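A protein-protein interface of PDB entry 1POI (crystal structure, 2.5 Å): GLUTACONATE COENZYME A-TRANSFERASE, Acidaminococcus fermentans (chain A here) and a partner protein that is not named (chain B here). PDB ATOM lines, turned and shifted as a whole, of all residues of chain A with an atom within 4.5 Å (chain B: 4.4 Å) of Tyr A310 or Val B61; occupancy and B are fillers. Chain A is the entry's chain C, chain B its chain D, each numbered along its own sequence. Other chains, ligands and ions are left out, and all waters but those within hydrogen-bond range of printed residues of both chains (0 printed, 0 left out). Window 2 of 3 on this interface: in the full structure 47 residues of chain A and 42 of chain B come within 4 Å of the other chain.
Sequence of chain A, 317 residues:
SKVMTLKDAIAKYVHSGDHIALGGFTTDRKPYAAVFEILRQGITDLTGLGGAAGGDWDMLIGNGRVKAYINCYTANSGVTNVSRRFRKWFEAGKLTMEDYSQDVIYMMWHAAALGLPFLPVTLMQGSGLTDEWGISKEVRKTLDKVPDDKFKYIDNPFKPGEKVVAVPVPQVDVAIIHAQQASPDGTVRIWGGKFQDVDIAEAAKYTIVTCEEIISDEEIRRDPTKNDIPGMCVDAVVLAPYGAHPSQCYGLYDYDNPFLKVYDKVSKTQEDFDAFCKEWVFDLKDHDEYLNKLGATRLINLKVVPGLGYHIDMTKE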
ATOM      1  N   ASP A 254     -24.845   1.758 -11.218  1.00  0.00           N
ATOM      2  CA  ASP A 254     -24.274   1.665 -12.551  1.00  0.00           C
ATOM      3  C   ASP A 254     -23.289   0.496 -12.587  1.00  0.00           C
ATOM      4  O   ASP A 254     -23.053  -0.129 -11.547  1.00  0.00           O
ATOM      5  CB  ASP A 254     -23.530   2.976 -12.841  1.00  0.00           C
ATOM      6  CG  ASP A 254     -23.441   3.285 -14.318  1.00  0.00           C
ATOM      7  OD1 ASP A 254     -23.809   2.402 -15.106  1.00  0.00           O
ATOM      8  OD2 ASP A 254     -23.003   4.403 -14.681  1.00  0.00           O
ATOM      9  N   VAL A 304     -26.384   5.645  -8.868  1.00  0.00           N
ATOM     10  CA  VAL A 304     -27.144   6.306  -9.907  1.00  0.00           C
ATOM     11  C   VAL A 304     -27.568   7.696  -9.442  1.00  0.00           C
ATOM     12  O   VAL A 304     -28.101   7.849  -8.351  1.00  0.00           O
ATOM     13  CB  VAL A 304     -28.374   5.432 -10.279  1.00  0.00           C
ATOM     14  CG1 VAL A 304     -29.443   6.239 -11.008  1.00  0.00           C
ATOM     15  CG2 VAL A 304     -27.917   4.264 -11.130  1.00  0.00           C
ATOM     16  N   VAL A 305     -27.270   8.707 -10.250  1.00  0.00           N
ATOM     17  CA  VAL A 305     -27.621  10.088  -9.943  1.00  0.00           C
ATOM     18  C   VAL A 305     -29.031  10.359 -10.436  1.00  0.00           C
ATOM     19  O   VAL A 305     -29.346  10.065 -11.595  1.00  0.00           O
ATOM     20  CB  VAL A 305     -26.693  11.054 -10.661  1.00  0.00           C
ATOM     21  CG1 VAL A 305     -27.141  12.460 -10.458  1.00  0.00           C
ATOM     22  CG2 VAL A 305     -25.305  10.881 -10.152  1.00  0.00           C
ATOM     23  N   LEU A 308     -30.138  11.541 -14.245  1.00  0.00           N
ATOM     24  CA  LEU A 308     -29.350  10.922 -15.301  1.00  0.00           C
ATOM     25  C   LEU A 308     -29.743   9.468 -15.405  1.00  0.00           C
ATOM     26  O   LEU A 308     -30.031   8.970 -16.489  1.00  0.00           O
ATOM     27  CB  LEU A 308     -27.866  10.999 -14.997  1.00  0.00           C
ATOM     28  CG  LEU A 308     -27.284  12.404 -15.036  1.00  0.00           C
ATOM     29  CD1 LEU A 308     -25.795  12.296 -14.896  1.00  0.00           C
ATOM     30  CD2 LEU A 308     -27.628  13.098 -16.341  1.00  0.00           C
ATOM     31  N   GLY A 309     -29.763   8.779 -14.273  1.00  0.00           N
ATOM     32  CA  GLY A 309     -30.129   7.377 -14.292  1.00  0.00           C
ATOM     33  C   GLY A 309     -28.886   6.523 -14.326  1.00  0.00           C
ATOM     34  O   GLY A 309     -28.960   5.293 -14.261  1.00  0.00           O
ATOM     35  N   TYR A 310     -27.735   7.179 -14.438  1.00  0.00           N
ATOM     36  CA  TYR A 310     -26.453   6.482 -14.462  1.00  0.00           C
ATOM     37  C   TYR A 310     -25.537   7.268 -13.527  1.00  0.00           C
ATOM     38  O   TYR A 310     -25.873   8.385 -13.143  1.00  0.00           O
ATOM     39  CB  TYR A 310     -25.883   6.381 -15.909  1.00  0.00           C
ATOM     40  CG  TYR A 310     -25.791   7.678 -16.716  1.00  0.00           C
ATOM     41  CD1 TYR A 310     -24.671   8.516 -16.619  1.00  0.00           C
ATOM     42  CD2 TYR A 310     -26.831   8.072 -17.572  1.00  0.00           C
ATOM     43  CE1 TYR A 310     -24.592   9.719 -17.346  1.00  0.00           C
ATOM     44  CE2 TYR A 310     -26.760   9.271 -18.315  1.00  0.00           C
ATOM     45  CZ  TYR A 310     -25.643  10.087 -18.194  1.00  0.00           C
ATOM     46  OH  TYR A 310     -25.579  11.269 -18.917  1.00  0.00           O
ATOM     47  N   HIS A 311     -24.387   6.716 -13.161  1.00  0.00           N
ATOM     48  CA  HIS A 311     -23.506   7.435 -12.252  1.00  0.00           C
ATOM     49  C   HIS A 311     -22.560   8.414 -12.906  1.00  0.00           C
ATOM     50  O   HIS A 311     -22.129   8.205 -14.029  1.00  0.00           O
ATOM     51  CB  HIS A 311     -22.675   6.456 -11.389  1.00  0.00           C
ATOM     52  CG  HIS A 311     -21.725   7.143 -10.444  1.00  0.00           C
ATOM     53  ND1 HIS A 311     -20.518   7.680 -10.856  1.00  0.00           N
ATOM     54  CD2 HIS A 311     -21.849   7.471  -9.136  1.00  0.00           C
ATOM     55  CE1 HIS A 311     -19.947   8.317  -9.849  1.00  0.00           C
ATOM     56  NE2 HIS A 311     -20.735   8.206  -8.794  1.00  0.00           N
ATOM     57  N   ILE A 312     -22.315   9.527 -12.224  1.00  0.00           N
ATOM     58  CA  ILE A 312     -21.310  10.496 -12.645  1.00  0.00           C
ATOM     59  C   ILE A 312     -20.872  11.143 -11.343  1.00  0.00           C
ATOM     60  O   ILE A 312     -21.471  10.886 -10.303  1.00  0.00           O
ATOM     61  CB  ILE A 312     -21.768  11.596 -13.632  1.00  0.00           C
ATOM     62  CG1 ILE A 312     -22.765  12.540 -12.982  1.00  0.00           C
ATOM     63  CG2 ILE A 312     -22.251  10.994 -14.930  1.00  0.00           C
ATOM     64  CD1 ILE A 312     -22.882  13.832 -13.725  1.00  0.00           C
ATOM     65  N   SER B  59     -32.787   9.054 -26.733  1.00  0.00           N
ATOM     66  CA  SER B  59     -32.067  10.317 -26.773  1.00  0.00           C
ATOM     67  C   SER B  59     -31.090  10.318 -25.591  1.00  0.00           C
ATOM     68  O   SER B  59     -31.348  10.907 -24.539  1.00  0.00           O
ATOM     69  CB  SER B  59     -33.029  11.501 -26.697  1.00  0.00           C
ATOM     70  OG  SER B  59     -32.305  12.724 -26.796  1.00  0.00           O
ATOM     71  N   PRO B  60     -29.933   9.671 -25.771  1.00  0.00           N
ATOM     72  CA  PRO B  60     -28.898   9.569 -24.739  1.00  0.00           C
ATOM     73  C   PRO B  60     -28.237  10.893 -24.451  1.00  0.00           C
ATOM     74  O   PRO B  60     -28.243  11.786 -25.294  1.00  0.00           O
ATOM     75  CB  PRO B  60     -27.883   8.601 -25.352  1.00  0.00           C
ATOM     76  CG  PRO B  60     -28.654   7.925 -26.507  1.00  0.00           C
ATOM     77  CD  PRO B  60     -29.475   9.058 -27.027  1.00  0.00           C
ATOM     78  N   VAL B  61     -27.696  11.018 -23.239  1.00  0.00           N
ATOM     79  CA  VAL B  61     -26.984  12.217 -22.819  1.00  0.00           C
ATOM     80  C   VAL B  61     -25.500  11.862 -22.980  1.00  0.00           C
ATOM     81  O   VAL B  61     -24.775  12.488 -23.761  1.00  0.00           O
ATOM     82  CB  VAL B  61     -27.297  12.585 -21.352  1.00  0.00           C
ATOM     83  CG1 VAL B  61     -26.366  13.690 -20.876  1.00  0.00           C
ATOM     84  CG2 VAL B  61     -28.730  13.058 -21.227  1.00  0.00           C
ATOM     85  N   GLU B  62     -25.062  10.852 -22.235  1.00  0.00           N
ATOM     86  CA  GLU B  62     -23.701  10.379 -22.313  1.00  0.00           C
ATOM     87  C   GLU B  62     -23.896   9.102 -23.084  1.00  0.00           C
ATOM     88  O   GLU B  62     -24.901   8.415 -22.891  1.00  0.00           O
ATOM     89  CB  GLU B  62     -23.149  10.064 -20.923  1.00  0.00           C
ATOM     90  CG  GLU B  62     -21.771   9.383 -20.948  1.00  0.00           C
ATOM     91  CD  GLU B  62     -21.323   8.902 -19.581  1.00  0.00           C
ATOM     92  OE1 GLU B  62     -20.838   9.736 -18.787  1.00  0.00           O
ATOM     93  OE2 GLU B  62     -21.470   7.695 -19.299  1.00  0.00           O
ATOM     94  N   VAL B  63     -22.931   8.775 -23.937  1.00  0.00           N
ATOM     95  CA  VAL B  63     -23.002   7.587 -24.785  1.00  0.00           C
ATOM     96  C   VAL B  63     -23.032   6.233 -24.100  1.00  0.00           C
ATOM     97  O   VAL B  63     -22.261   5.968 -23.180  1.00  0.00           O
ATOM     98  CB  VAL B  63     -21.876   7.565 -25.897  1.00  0.00           C
ATOM     99  CG1 VAL B  63     -22.288   8.419 -27.095  1.00  0.00           C
ATOM    100  CG2 VAL B  63     -20.537   8.063 -25.341  1.00  0.00           C
ATOM    101  N   ARG B  71     -27.896   4.216 -19.858  1.00  0.00           N
ATOM    102  CA  ARG B  71     -27.677   5.470 -20.571  1.00  0.00           C
ATOM    103  C   ARG B  71     -28.703   5.662 -21.716  1.00  0.00           C
ATOM    104  O   ARG B  71     -28.932   6.783 -22.185  1.00  0.00           O
ATOM    105  CB  ARG B  71     -26.228   5.531 -21.053  1.00  0.00           C
ATOM    106  CG  ARG B  71     -25.372   6.544 -20.321  1.00  0.00           C
ATOM    107  CD  ARG B  71     -23.945   6.070 -20.185  1.00  0.00           C
ATOM    108  NE  ARG B  71     -23.976   4.842 -19.424  1.00  0.00           N
ATOM    109  CZ  ARG B  71     -23.439   4.690 -18.218  1.00  0.00           C
ATOM    110  NH1 ARG B  71     -22.756   5.667 -17.628  1.00  0.00           N
ATOM    111  NH2 ARG B  71     -23.825   3.643 -17.498  1.00  0.00           N
ATOM    112  N   HIS B  75     -33.176   7.291 -20.778  1.00  0.00           N
ATOM    113  CA  HIS B  75     -33.354   8.369 -21.746  1.00  0.00           C
ATOM    114  C   HIS B  75     -34.031   7.950 -23.033  1.00  0.00           C
ATOM    115  O   HIS B  75     -33.469   8.069 -24.120  1.00  0.00           O
ATOM    116  CB  HIS B  75     -32.020   9.022 -22.061  1.00  0.00           C
ATOM    117  CG  HIS B  75     -31.461   9.813 -20.930  1.00  0.00           C
ATOM    118  ND1 HIS B  75     -31.420  11.190 -20.933  1.00  0.00           N
ATOM    119  CD2 HIS B  75     -30.919   9.423 -19.755  1.00  0.00           C
ATOM    120  CE1 HIS B  75     -30.880  11.614 -19.806  1.00  0.00           C
ATOM    121  NE2 HIS B  75     -30.566  10.560 -19.074  1.00  0.00           N
ATOM    122  N   GLU B 249     -19.484  17.107 -26.996  1.00  0.00           N
ATOM    123  CA  GLU B 249     -20.822  16.834 -26.469  1.00  0.00           C
ATOM    124  C   GLU B 249     -21.261  15.399 -26.653  1.00  0.00           C
ATOM    125  O   GLU B 249     -21.756  14.774 -25.708  1.00  0.00           O
ATOM    126  CB  GLU B 249     -21.883  17.741 -27.086  1.00  0.00           C
ATOM    127  CG  GLU B 249     -22.121  19.037 -26.342  1.00  0.00           C
ATOM    128  CD  GLU B 249     -21.659  20.249 -27.133  1.00  0.00           C
ATOM    129  OE1 GLU B 249     -20.491  20.258 -27.591  1.00  0.00           O
ATOM    130  OE2 GLU B 249     -22.460  21.195 -27.300  1.00  0.00           O
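A ring nitrogen (NE2) of His B75 sits at hydrogen-bond distance from the backbone carbonyl oxygen (O) of Leu A308 (3.1 Å). N of Glu B62 lies close to OH of Tyr A310 (3.4 Å). The side-chain carboxylate (OD1) of Asp A254 is in salt-bridge range of the guanidinium group (NH2) of Arg B71, 2.7 Å away.
The side-chain carboxylate of Asp A254 sits at hydrogen-bond distance from the backbone NH of His A311 (3.1 Å). The backbone NH of Val A305 is in hydrogen-bond range of the backbone carbonyl oxygen of Tyr A310. OE2 of Glu B62 is in salt-bridge range of NH1 of Arg B71 (2.9 Å). The backbone carbonyl oxygen (O) of His B75 lies within hydrogen-bond range of the backbone NH (N) of Ser B59, 2.9 Å away.
Among the printed residues, merely in contact across the chains: Tyr A310 with Val B61 and Tyr A310 with Arg B71.
Of the printed residues of chain B, Tyr A310 touches Val B61, Glu B62 and Arg B71. Val B61 touches just one residue of chain A: Tyr A310 (3.2 Å). Of the printed residues of chain A, Glu B62 touches Tyr A310 (3.4 Å). Of the printed residues of chain B, Asp A254 touches Arg B71. The nearest printed residue of chain A that does not touch Val B61 is Leu A308 (4.7 Å). The nearest printed residue of chain A that does not touch Arg B71 is His A311 (4.4 Å).
Printed residues of chain B that touch a printed residue of chain A: Val B61, Glu B62, Arg B71 and His B75. Hydrophobic or aromatic side chains of chain B that line the printed part of chain A: Val B61 and His B75.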
